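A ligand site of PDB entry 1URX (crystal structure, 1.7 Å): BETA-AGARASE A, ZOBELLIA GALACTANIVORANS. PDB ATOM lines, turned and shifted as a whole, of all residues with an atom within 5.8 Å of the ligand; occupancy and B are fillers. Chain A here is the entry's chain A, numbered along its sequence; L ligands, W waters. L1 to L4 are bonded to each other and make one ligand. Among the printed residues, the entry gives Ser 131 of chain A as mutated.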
ATOM      1  N   TYR A  53      27.006 -18.628   2.833  1.00  0.00           N
ATOM      2  CA  TYR A  53      27.148 -18.281   4.257  1.00  0.00           C
ATOM      3  C   TYR A  53      28.580 -18.522   4.682  1.00  0.00           C
ATOM      4  O   TYR A  53      29.383 -19.067   3.900  1.00  0.00           O
ATOM      5  CB  TYR A  53      26.124 -19.047   5.066  1.00  0.00           C
ATOM      6  CG  TYR A  53      26.115 -18.774   6.554  1.00  0.00           C
ATOM      7  CD1 TYR A  53      25.734 -17.531   7.033  1.00  0.00           C
ATOM      8  CD2 TYR A  53      26.401 -19.785   7.478  1.00  0.00           C
ATOM      9  CE1 TYR A  53      25.715 -17.255   8.379  1.00  0.00           C
ATOM     10  CE2 TYR A  53      26.389 -19.527   8.847  1.00  0.00           C
ATOM     11  CZ  TYR A  53      26.052 -18.254   9.291  1.00  0.00           C
ATOM     12  OH  TYR A  53      26.032 -17.989  10.629  1.00  0.00           O
ATOM     13  N   ASN A  55      29.848 -20.545   6.738  1.00  0.00           N
ATOM     14  CA  ASN A  55      30.108 -21.965   6.941  1.00  0.00           C
ATOM     15  C   ASN A  55      28.946 -22.739   6.271  1.00  0.00           C
ATOM     16  O   ASN A  55      28.183 -22.144   5.502  1.00  0.00           O
ATOM     17  CB  ASN A  55      30.303 -22.298   8.433  1.00  0.00           C
ATOM     18  CG  ASN A  55      29.105 -21.924   9.297  1.00  0.00           C
ATOM     19  OD1 ASN A  55      27.988 -22.281   8.975  1.00  0.00           O
ATOM     20  ND2 ASN A  55      29.348 -21.253  10.434  1.00  0.00           N
ATOM     21  N   GLY A  56      28.839 -24.037   6.576  1.00  0.00           N
ATOM     22  CA  GLY A  56      27.862 -24.940   5.959  1.00  0.00           C
ATOM     23  C   GLY A  56      26.384 -24.761   6.320  1.00  0.00           C
ATOM     24  O   GLY A  56      25.511 -25.404   5.697  1.00  0.00           O
ATOM     25  N   TRP A  57      26.063 -23.924   7.316  1.00  0.00           N
ATOM     26  CA  TRP A  57      24.668 -23.729   7.724  1.00  0.00           C
ATOM     27  C   TRP A  57      23.877 -23.187   6.529  1.00  0.00           C
ATOM     28  O   TRP A  57      24.376 -22.352   5.813  1.00  0.00           O
ATOM     29  CB  TRP A  57      24.604 -22.707   8.831  1.00  0.00           C
ATOM     30  CG  TRP A  57      23.300 -22.520   9.490  1.00  0.00           C
ATOM     31  CD1 TRP A  57      22.512 -23.479  10.067  1.00  0.00           C
ATOM     32  CD2 TRP A  57      22.658 -21.263   9.741  1.00  0.00           C
ATOM     33  NE1 TRP A  57      21.411 -22.895  10.629  1.00  0.00           N
ATOM     34  CE2 TRP A  57      21.476 -21.533  10.458  1.00  0.00           C
ATOM     35  CE3 TRP A  57      22.970 -19.941   9.438  1.00  0.00           C
ATOM     36  CZ2 TRP A  57      20.600 -20.531  10.858  1.00  0.00           C
ATOM     37  CZ3 TRP A  57      22.085 -18.928   9.838  1.00  0.00           C
ATOM     38  CH2 TRP A  57      20.918 -19.240  10.550  1.00  0.00           C
ATOM     39  N   PRO A  60      18.026 -20.096   8.747  1.00  0.00           N
ATOM     40  CA  PRO A  60      17.037 -20.366   9.793  1.00  0.00           C
ATOM     41  C   PRO A  60      15.670 -20.696   9.200  1.00  0.00           C
ATOM     42  O   PRO A  60      15.360 -20.255   8.099  1.00  0.00           O
ATOM     43  CB  PRO A  60      16.990 -19.046  10.558  1.00  0.00           C
ATOM     44  CG  PRO A  60      17.209 -18.028   9.490  1.00  0.00           C
ATOM     45  CD  PRO A  60      18.162 -18.651   8.503  1.00  0.00           C
ATOM     46  N   ALA A 118      12.866 -11.666   5.503  1.00  0.00           N
ATOM     47  CA  ALA A 118      13.871 -10.702   5.919  1.00  0.00           C
ATOM     48  C   ALA A 118      14.884 -10.394   4.798  1.00  0.00           C
ATOM     49  O   ALA A 118      15.270 -11.281   4.029  1.00  0.00           O
ATOM     50  CB  ALA A 118      14.620 -11.183   7.147  1.00  0.00           C
ATOM     51  N   ALA A 120      18.681  -8.419   4.910  1.00  0.00           N
ATOM     52  CA  ALA A 120      19.604  -7.869   5.877  1.00  0.00           C
ATOM     53  C   ALA A 120      21.017  -7.606   5.338  1.00  0.00           C
ATOM     54  O   ALA A 120      21.481  -8.277   4.428  1.00  0.00           O
ATOM     55  CB  ALA A 120      19.632  -8.775   7.106  1.00  0.00           C
ATOM     56  N   TRP A 122      24.579  -7.193   7.447  1.00  0.00           N
ATOM     57  CA  TRP A 122      24.998  -7.502   8.801  1.00  0.00           C
ATOM     58  C   TRP A 122      26.398  -8.061   8.865  1.00  0.00           C
ATOM     59  O   TRP A 122      26.982  -8.346   7.841  1.00  0.00           O
ATOM     60  CB  TRP A 122      24.040  -8.454   9.492  1.00  0.00           C
ATOM     61  CG  TRP A 122      23.687  -9.753   8.803  1.00  0.00           C
ATOM     62  CD1 TRP A 122      23.090  -9.882   7.572  1.00  0.00           C
ATOM     63  CD2 TRP A 122      23.809 -11.082   9.319  1.00  0.00           C
ATOM     64  NE1 TRP A 122      22.876 -11.207   7.277  1.00  0.00           N
ATOM     65  CE2 TRP A 122      23.306 -11.974   8.338  1.00  0.00           C
ATOM     66  CE3 TRP A 122      24.288 -11.623  10.521  1.00  0.00           C
ATOM     67  CZ2 TRP A 122      23.269 -13.347   8.530  1.00  0.00           C
ATOM     68  CZ3 TRP A 122      24.243 -12.985  10.712  1.00  0.00           C
ATOM     69  CH2 TRP A 122      23.715 -13.832   9.735  1.00  0.00           C
ATOM     70  N   THR A 123      26.973  -8.095  10.068  1.00  0.00           N
ATOM     71  CA  THR A 123      28.238  -8.770  10.271  1.00  0.00           C
ATOM     72  C   THR A 123      28.053  -9.986  11.193  1.00  0.00           C
ATOM     73  O   THR A 123      27.089 -10.060  11.980  1.00  0.00           O
ATOM     74  CB  THR A 123      29.255  -7.866  10.867  1.00  0.00           C
ATOM     75  OG1 THR A 123      28.857  -7.483  12.187  1.00  0.00           O
ATOM     76  CG2 THR A 123      29.434  -6.541  10.072  1.00  0.00           C
ATOM     77  N   LEU A 124      28.968 -10.932  11.086  1.00  0.00           N
ATOM     78  CA  LEU A 124      28.993 -12.089  11.965  1.00  0.00           C
ATOM     79  C   LEU A 124      30.401 -12.664  11.991  1.00  0.00           C
ATOM     80  O   LEU A 124      30.995 -12.870  10.956  1.00  0.00           O
ATOM     81  CB  LEU A 124      28.050 -13.198  11.506  1.00  0.00           C
ATOM     82  CG  LEU A 124      27.831 -14.372  12.473  1.00  0.00           C
ATOM     83  CD1 LEU A 124      27.188 -13.929  13.780  1.00  0.00           C
ATOM     84  CD2 LEU A 124      27.023 -15.448  11.795  1.00  0.00           C
ATOM     85  N   GLU A 128      30.722 -16.978  15.541  1.00  0.00           N
ATOM     86  CA  GLU A 128      29.280 -16.744  15.591  1.00  0.00           C
ATOM     87  C   GLU A 128      28.811 -16.128  16.912  1.00  0.00           C
ATOM     88  O   GLU A 128      27.610 -16.144  17.222  1.00  0.00           O
ATOM     89  CB  GLU A 128      28.453 -17.972  15.196  1.00  0.00           C
ATOM     90  CG  GLU A 128      28.739 -18.444  13.779  1.00  0.00           C
ATOM     91  CD  GLU A 128      28.055 -19.733  13.369  1.00  0.00           C
ATOM     92  OE1 GLU A 128      27.402 -19.756  12.276  1.00  0.00           O
ATOM     93  OE2 GLU A 128      28.189 -20.740  14.104  1.00  0.00           O
ATOM     94  N   SER A 131      27.462 -10.120  16.338  1.00  0.00           N
ATOM     95  CA  SER A 131      26.789  -9.669  15.112  1.00  0.00           C
ATOM     96  C   SER A 131      26.312  -8.223  15.194  1.00  0.00           C
ATOM     97  O   SER A 131      25.807  -7.796  16.218  1.00  0.00           O
ATOM     98  CB  SER A 131      25.629 -10.599  14.796  1.00  0.00           C
ATOM     99  OG  SER A 131      24.975 -10.159  13.662  1.00  0.00           O
ATOM    100  N   ASP A 133      23.659  -5.761  13.028  1.00  0.00           N
ATOM    101  CA  ASP A 133      22.671  -5.644  11.964  1.00  0.00           C
ATOM    102  C   ASP A 133      22.564  -4.204  11.524  1.00  0.00           C
ATOM    103  O   ASP A 133      21.864  -3.407  12.160  1.00  0.00           O
ATOM    104  CB  ASP A 133      21.297  -6.147  12.423  1.00  0.00           C
ATOM    105  CG  ASP A 133      21.349  -7.548  12.950  1.00  0.00           C
ATOM    106  OD1 ASP A 133      21.959  -8.418  12.286  1.00  0.00           O
ATOM    107  OD2 ASP A 133      20.815  -7.883  14.025  1.00  0.00           O
ATOM    108  N   GLU A 136      17.842  -4.607   8.833  1.00  0.00           N
ATOM    109  CA  GLU A 136      17.103  -5.863   8.692  1.00  0.00           C
ATOM    110  C   GLU A 136      15.665  -5.434   8.454  1.00  0.00           C
ATOM    111  O   GLU A 136      15.047  -4.867   9.350  1.00  0.00           O
ATOM    112  CB  GLU A 136      17.236  -6.740   9.935  1.00  0.00           C
ATOM    113  CG  GLU A 136      16.532  -8.117   9.839  1.00  0.00           C
ATOM    114  CD  GLU A 136      16.706  -8.992  11.061  1.00  0.00           C
ATOM    115  OE1 GLU A 136      16.855 -10.243  10.900  1.00  0.00           O
ATOM    116  OE2 GLU A 136      16.653  -8.432  12.219  1.00  0.00           O
ATOM    117  N   TYR A 138      11.660  -6.000   6.374  1.00  0.00           N
ATOM    118  CA  TYR A 138      10.616  -6.965   6.060  1.00  0.00           C
ATOM    119  C   TYR A 138       9.592  -6.207   5.194  1.00  0.00           C
ATOM    120  O   TYR A 138       8.772  -5.469   5.730  1.00  0.00           O
ATOM    121  CB  TYR A 138       9.927  -7.499   7.325  1.00  0.00           C
ATOM    122  CG  TYR A 138      10.902  -8.175   8.302  1.00  0.00           C
ATOM    123  CD1 TYR A 138      11.709  -7.422   9.154  1.00  0.00           C
ATOM    124  CD2 TYR A 138      11.055  -9.550   8.289  1.00  0.00           C
ATOM    125  CE1 TYR A 138      12.618  -8.056  10.005  1.00  0.00           C
ATOM    126  CE2 TYR A 138      11.934 -10.183   9.111  1.00  0.00           C
ATOM    127  CZ  TYR A 138      12.722  -9.432  10.003  1.00  0.00           C
ATOM    128  OH  TYR A 138      13.653 -10.052  10.832  1.00  0.00           O
ATOM    129  N   HIS A 156      23.676  -8.418  17.929  1.00  0.00           N
ATOM    130  CA  HIS A 156      23.529  -9.581  18.823  1.00  0.00           C
ATOM    131  C   HIS A 156      24.820  -9.988  19.454  1.00  0.00           C
ATOM    132  O   HIS A 156      25.882  -9.792  18.911  1.00  0.00           O
ATOM    133  CB  HIS A 156      22.945 -10.789  18.056  1.00  0.00           C
ATOM    134  CG  HIS A 156      21.594 -10.532  17.456  1.00  0.00           C
ATOM    135  ND1 HIS A 156      20.447 -11.147  17.905  1.00  0.00           N
ATOM    136  CD2 HIS A 156      21.208  -9.748  16.412  1.00  0.00           C
ATOM    137  CE1 HIS A 156      19.408 -10.743  17.187  1.00  0.00           C
ATOM    138  NE2 HIS A 156      19.848  -9.885  16.278  1.00  0.00           N
ATOM    139  N   PHE A 158      26.017 -13.634  21.404  1.00  0.00           N
ATOM    140  CA  PHE A 158      25.579 -14.998  21.583  1.00  0.00           C
ATOM    141  C   PHE A 158      26.536 -15.806  22.467  1.00  0.00           C
ATOM    142  O   PHE A 158      27.764 -15.669  22.402  1.00  0.00           O
ATOM    143  CB  PHE A 158      25.501 -15.786  20.267  1.00  0.00           C
ATOM    144  CG  PHE A 158      24.661 -15.156  19.152  1.00  0.00           C
ATOM    145  CD1 PHE A 158      25.235 -14.352  18.196  1.00  0.00           C
ATOM    146  CD2 PHE A 158      23.298 -15.473  19.041  1.00  0.00           C
ATOM    147  CE1 PHE A 158      24.463 -13.819  17.184  1.00  0.00           C
ATOM    148  CE2 PHE A 158      22.543 -14.963  18.021  1.00  0.00           C
ATOM    149  CZ  PHE A 158      23.132 -14.127  17.091  1.00  0.00           C
ATOM    150  N   ARG A 160      27.068 -19.845  22.152  1.00  0.00           N
ATOM    151  CA  ARG A 160      26.711 -20.858  21.163  1.00  0.00           C
ATOM    152  C   ARG A 160      26.105 -22.123  21.757  1.00  0.00           C
ATOM    153  O   ARG A 160      25.201 -22.696  21.166  1.00  0.00           O
ATOM    154  CB  ARG A 160      27.891 -21.211  20.277  1.00  0.00           C
ATOM    155  CG  ARG A 160      28.491 -19.994  19.548  1.00  0.00           C
ATOM    156  CD  ARG A 160      27.475 -19.099  18.866  1.00  0.00           C
ATOM    157  NE  ARG A 160      26.607 -19.849  17.985  1.00  0.00           N
ATOM    158  CZ  ARG A 160      25.605 -19.314  17.290  1.00  0.00           C
ATOM    159  NH1 ARG A 160      25.358 -18.035  17.338  1.00  0.00           N
ATOM    160  NH2 ARG A 160      24.843 -20.106  16.574  1.00  0.00           N
ATOM    161  N   PHE A 163      22.682 -22.438  23.153  1.00  0.00           N
ATOM    162  CA  PHE A 163      22.366 -21.268  22.319  1.00  0.00           C
ATOM    163  C   PHE A 163      21.606 -20.235  23.137  1.00  0.00           C
ATOM    164  O   PHE A 163      20.522 -20.523  23.662  1.00  0.00           O
ATOM    165  CB  PHE A 163      21.574 -21.659  21.076  1.00  0.00           C
ATOM    166  CG  PHE A 163      21.259 -20.489  20.171  1.00  0.00           C
ATOM    167  CD1 PHE A 163      22.231 -19.965  19.335  1.00  0.00           C
ATOM    168  CD2 PHE A 163      20.011 -19.923  20.153  1.00  0.00           C
ATOM    169  CE1 PHE A 163      21.956 -18.872  18.500  1.00  0.00           C
ATOM    170  CE2 PHE A 163      19.716 -18.829  19.309  1.00  0.00           C
ATOM    171  CZ  PHE A 163      20.696 -18.325  18.475  1.00  0.00           C
ATOM    172  N   ASP A 165      20.747 -15.898  22.865  1.00  0.00           N
ATOM    173  CA  ASP A 165      20.761 -14.761  21.957  1.00  0.00           C
ATOM    174  C   ASP A 165      20.313 -13.498  22.668  1.00  0.00           C
ATOM    175  O   ASP A 165      19.164 -13.423  23.106  1.00  0.00           O
ATOM    176  CB  ASP A 165      19.803 -15.107  20.813  1.00  0.00           C
ATOM    177  CG  ASP A 165      19.678 -14.018  19.794  1.00  0.00           C
ATOM    178  OD1 ASP A 165      20.423 -13.024  19.879  1.00  0.00           O
ATOM    179  OD2 ASP A 165      18.830 -14.074  18.861  1.00  0.00           O
ATOM    180  N   ASP A 236      22.063 -10.812   2.864  1.00  0.00           N
ATOM    181  CA  ASP A 236      21.248 -12.025   2.587  1.00  0.00           C
ATOM    182  C   ASP A 236      19.741 -11.749   2.664  1.00  0.00           C
ATOM    183  O   ASP A 236      19.305 -10.616   2.947  1.00  0.00           O
ATOM    184  CB  ASP A 236      21.626 -13.258   3.469  1.00  0.00           C
ATOM    185  CG  ASP A 236      21.065 -13.199   4.875  1.00  0.00           C
ATOM    186  OD1 ASP A 236      20.673 -12.117   5.356  1.00  0.00           O
ATOM    187  OD2 ASP A 236      21.056 -14.218   5.605  1.00  0.00           O
ATOM    188  N   GLU A 238      16.227 -14.087   4.208  1.00  0.00           N
ATOM    189  CA  GLU A 238      15.911 -15.224   5.051  1.00  0.00           C
ATOM    190  C   GLU A 238      14.397 -15.395   5.197  1.00  0.00           C
ATOM    191  O   GLU A 238      13.670 -14.397   5.262  1.00  0.00           O
ATOM    192  CB  GLU A 238      16.530 -15.084   6.452  1.00  0.00           C
ATOM    193  CG  GLU A 238      18.060 -15.104   6.422  1.00  0.00           C
ATOM    194  CD  GLU A 238      18.688 -14.738   7.773  1.00  0.00           C
ATOM    195  OE1 GLU A 238      17.991 -14.702   8.802  1.00  0.00           O
ATOM    196  OE2 GLU A 238      19.917 -14.441   7.758  1.00  0.00           O
ATOM    197  N   GLN A 240      12.170 -16.398   7.838  1.00  0.00           N
ATOM    198  CA  GLN A 240      12.357 -16.556   9.258  1.00  0.00           C
ATOM    199  C   GLN A 240      11.105 -17.057   9.926  1.00  0.00           C
ATOM    200  O   GLN A 240      10.522 -16.371  10.755  1.00  0.00           O
ATOM    201  CB  GLN A 240      12.828 -15.200   9.886  1.00  0.00           C
ATOM    202  CG  GLN A 240      14.178 -14.726   9.340  1.00  0.00           C
ATOM    203  CD  GLN A 240      14.591 -13.349   9.836  1.00  0.00           C
ATOM    204  OE1 GLN A 240      15.770 -12.970   9.710  1.00  0.00           O
ATOM    205  NE2 GLN A 240      13.669 -12.631  10.426  1.00  0.00           N
HETATM  206  C1  LIG L   1      20.248 -11.366  13.075  1.00  0.00           C
HETATM  207  C2  LIG L   1      20.343 -12.817  13.497  1.00  0.00           C
HETATM  208  C3  LIG L   1      20.921 -13.768  12.430  1.00  0.00           C
HETATM  209  C4  LIG L   1      20.285 -13.495  11.055  1.00  0.00           C
HETATM  210  C5  LIG L   1      20.504 -12.031  10.726  1.00  0.00           C
HETATM  211  C6  LIG L   1      20.016 -11.556   9.332  1.00  0.00           C
HETATM  212  O1  LIG L   1      21.607 -11.063  12.855  1.00  0.00           O
HETATM  213  O2  LIG L   1      20.994 -12.892  14.774  1.00  0.00           O
HETATM  214  O3  LIG L   1      20.650 -15.089  12.862  1.00  0.00           O
HETATM  215  O4  LIG L   1      18.906 -13.864  11.143  1.00  0.00           O
HETATM  216  O5  LIG L   1      20.013 -11.113  11.705  1.00  0.00           O
HETATM  217  O6  LIG L   1      18.604 -11.629   9.250  1.00  0.00           O
HETATM  218  C1  LG2 L   2      21.793 -15.696  13.302  1.00  0.00           C
HETATM  219  C2  LG2 L   2      21.258 -16.892  14.107  1.00  0.00           C
HETATM  220  C3  LG2 L   2      22.346 -17.847  14.633  1.00  0.00           C
HETATM  221  C4  LG2 L   2      23.078 -18.381  13.488  1.00  0.00           C
HETATM  222  C5  LG2 L   2      23.688 -17.167  12.891  1.00  0.00           C
HETATM  223  C6  LG2 L   2      24.330 -16.689  14.186  1.00  0.00           C
HETATM  224  O1  LG2 L   2      20.149 -17.573  13.574  1.00  0.00           O
HETATM  225  O2  LG2 L   2      23.440 -17.133  15.242  1.00  0.00           O
HETATM  226  O3  LG2 L   2      24.020 -19.431  13.395  1.00  0.00           O
HETATM  227  O4  LG2 L   2      22.781 -16.132  12.380  1.00  0.00           O
HETATM  228  C1  LG3 L   3      23.497 -20.665  13.478  1.00  0.00           C
HETATM  229  C2  LG3 L   3      24.686 -21.600  13.344  1.00  0.00           C
HETATM  230  C3  LG3 L   3      24.311 -23.095  13.509  1.00  0.00           C
HETATM  231  C4  LG3 L   3      23.463 -23.293  14.774  1.00  0.00           C
HETATM  232  C5  LG3 L   3      22.284 -22.284  14.787  1.00  0.00           C
HETATM  233  C6  LG3 L   3      21.514 -22.354  16.094  1.00  0.00           C
HETATM  234  O1  LG3 L   3      25.342 -21.402  12.123  1.00  0.00           O
HETATM  235  O2  LG3 L   3      25.521 -23.799  13.678  1.00  0.00           O
HETATM  236  O3  LG3 L   3      24.207 -23.045  15.967  1.00  0.00           O
HETATM  237  O4  LG3 L   3      22.769 -20.951  14.651  1.00  0.00           O
HETATM  238  O5  LG3 L   3      20.262 -21.741  15.969  1.00  0.00           O
HETATM  239  C1  LG4 L   4      26.042 -24.488  12.537  1.00  0.00           C
HETATM  240  C2  LG4 L   4      27.327 -23.812  11.996  1.00  0.00           C
HETATM  241  C3  LG4 L   4      28.176 -24.786  11.169  1.00  0.00           C
HETATM  242  C4  LG4 L   4      28.453 -26.086  11.829  1.00  0.00           C
HETATM  243  C5  LG4 L   4      27.057 -26.588  11.975  1.00  0.00           C
HETATM  244  C6  LG4 L   4      26.611 -26.403  10.508  1.00  0.00           C
HETATM  245  O1  LG4 L   4      28.135 -23.296  13.051  1.00  0.00           O
HETATM  246  O2  LG4 L   4      27.376 -25.241  10.045  1.00  0.00           O
HETATM  247  O3  LG4 L   4      29.385 -27.211  11.625  1.00  0.00           O
HETATM  248  O4  LG4 L   4      26.257 -25.866  12.936  1.00  0.00           O
HETATM  249  O   HOH W   1      16.985 -12.325  12.565  1.00  0.00           O
HETATM  250  O   HOH W   2      17.960 -11.761   6.366  1.00  0.00           O
HETATM  251  O   HOH W   3      18.092 -21.744  13.262  1.00  0.00           O
HETATM  252  O   HOH W   4      30.796 -23.401  13.543  1.00  0.00           O
HETATM  253  O   HOH W   5      24.387 -27.343  14.372  1.00  0.00           O
HETATM  254  O   HOH W   6      17.846  -9.330  14.552  1.00  0.00           O
HETATM  255  O   HOH W   7      19.045 -13.887  16.158  1.00  0.00           O
HETATM  256  O   HOH W   8      18.098 -16.170  12.505  1.00  0.00           O
HETATM  257  O   HOH W   9      19.042 -19.757  14.724  1.00  0.00           O
HETATM  258  O   HOH W  10      29.845 -25.978   8.536  1.00  0.00           O
HETATM  259  O   HOH W  11      24.875 -22.876  18.614  1.00  0.00           O
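O1 of LG3 L3 is in hydrogen-bond range of OE1 of Glu 128 (2.6 Å). The side-chain carboxylate (OE1) of Glu 238 sits at hydrogen-bond distance from an oxygen (O4) of LIG L1, at 2.6 Å. An oxygen (O1) of LIG L1 sits at hydrogen-bond distance from the side-chain carboxylate (OD1) of Asp 133. The side-chain carboxylate (OE1) of Glu 136 sits at hydrogen-bond distance from an oxygen (O6) of LIG L1 (2.8 Å). NH2 of Arg 160 sits at hydrogen-bond distance from O4 of LG3 L3 (3.0 Å). OE1 of Gln 240 sits at hydrogen-bond distance from O6 of LIG L1 (3.2 Å). The side-chain amide oxygen (OD1) of Asn 55 lies close to an oxygen (O2) of LG4 L4, 3.2 Å away. N of Trp 57 is in hydrogen-bond range of O2 of LG4 L4, 3.3 Å away.
OE1 of Glu 128 lies within hydrogen-bond range of ND2 of Asn 55 (3.1 Å). The side-chain hydroxyl of Tyr 53 sits at hydrogen-bond distance from the side-chain carboxylate of Glu 128 (2.8 Å). The side-chain carboxylate of Glu 136 sits at hydrogen-bond distance from the side-chain hydroxyl of Tyr 138 (3.2 Å). The side-chain hydroxyl (OH) of Tyr 138 sits at hydrogen-bond distance from the side-chain amide nitrogen (NE2) of Gln 240 (2.6 Å). N of Trp 57 sits at hydrogen-bond distance from OD1 of Asn 55. NE1 of Trp 122 is in hydrogen-bond range of OD1 of Asp 236, at 3.1 Å. OG of Ser 131 lies within hydrogen-bond range of O of Thr 123, 2.7 Å away. O of Asp 236 sits at hydrogen-bond distance from N of Ala 120 (3.0 Å).
OH of Tyr 53 touches C5 of LG2 L2, at 3.4 Å. C of Gly 56 touches O2 of LG4 L4, 3.9 Å away. CB of Ala 120 touches C6 of LIG L1 (3.6 Å). CE2 of Trp 122 touches C6 of LIG L1 (3.5 Å). CD2 of Leu 124 touches C6 of LG2 L2 (3.8 Å). OG of Ser 131 touches O1 of LIG L1, at 3.6 Å. His 156 touches the ligand. CZ of Phe 158 touches O2 of LIG L1 (3.4 Å). CE1 of Phe 163 touches O2 of LG2 L2, 3.98 Å away. Hydrophobic or aromatic side chains that line the ligand: Tyr 53, Trp 57, Ala 120, Trp 122, Leu 124, His 156, Phe 158 and Phe 163. 17 residues have an atom within 4 Å of the ligand: Tyr 53, Asn 55, Gly 56, Trp 57, Ala 120, Trp 122, Leu 124, Glu 128, Ser 131, Asp 133, Glu 136, His 156, Phe 158, Arg 160, Phe 163, Glu 238 and Gln 240. The nearest printed residue that does not touch the ligand is Asp 236 (4.1 Å).
Water W7 bridges O2 of LIG L1 and OD2 of Asp 165. Water W11 lies within hydrogen-bond range of the backbone carbonyl oxygen of Arg 160 (2.6 Å) and an oxygen (O3) of LG3 L3 (2.7 Å). Water W1 lies within hydrogen-bond range of OE1 of Glu 136 (2.7 Å), O4 of LIG L1 (2.8 Å) and OE1 of Gln 240 (3.2 Å). Water W2 bridges the side-chain carboxylate (OD1) of Asp 236 (2.9 Å) and an oxygen (O6) of LIG L1 (3.0 Å). Water W10 lies within hydrogen-bond range of N of Gly 56 and O2 of LG4 L4. Water W6 lies within hydrogen-bond range of NE2 of His 156 (2.7 Å), OE2 of Glu 136 (2.8 Å) and OD2 of Asp 133 (3.3 Å).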
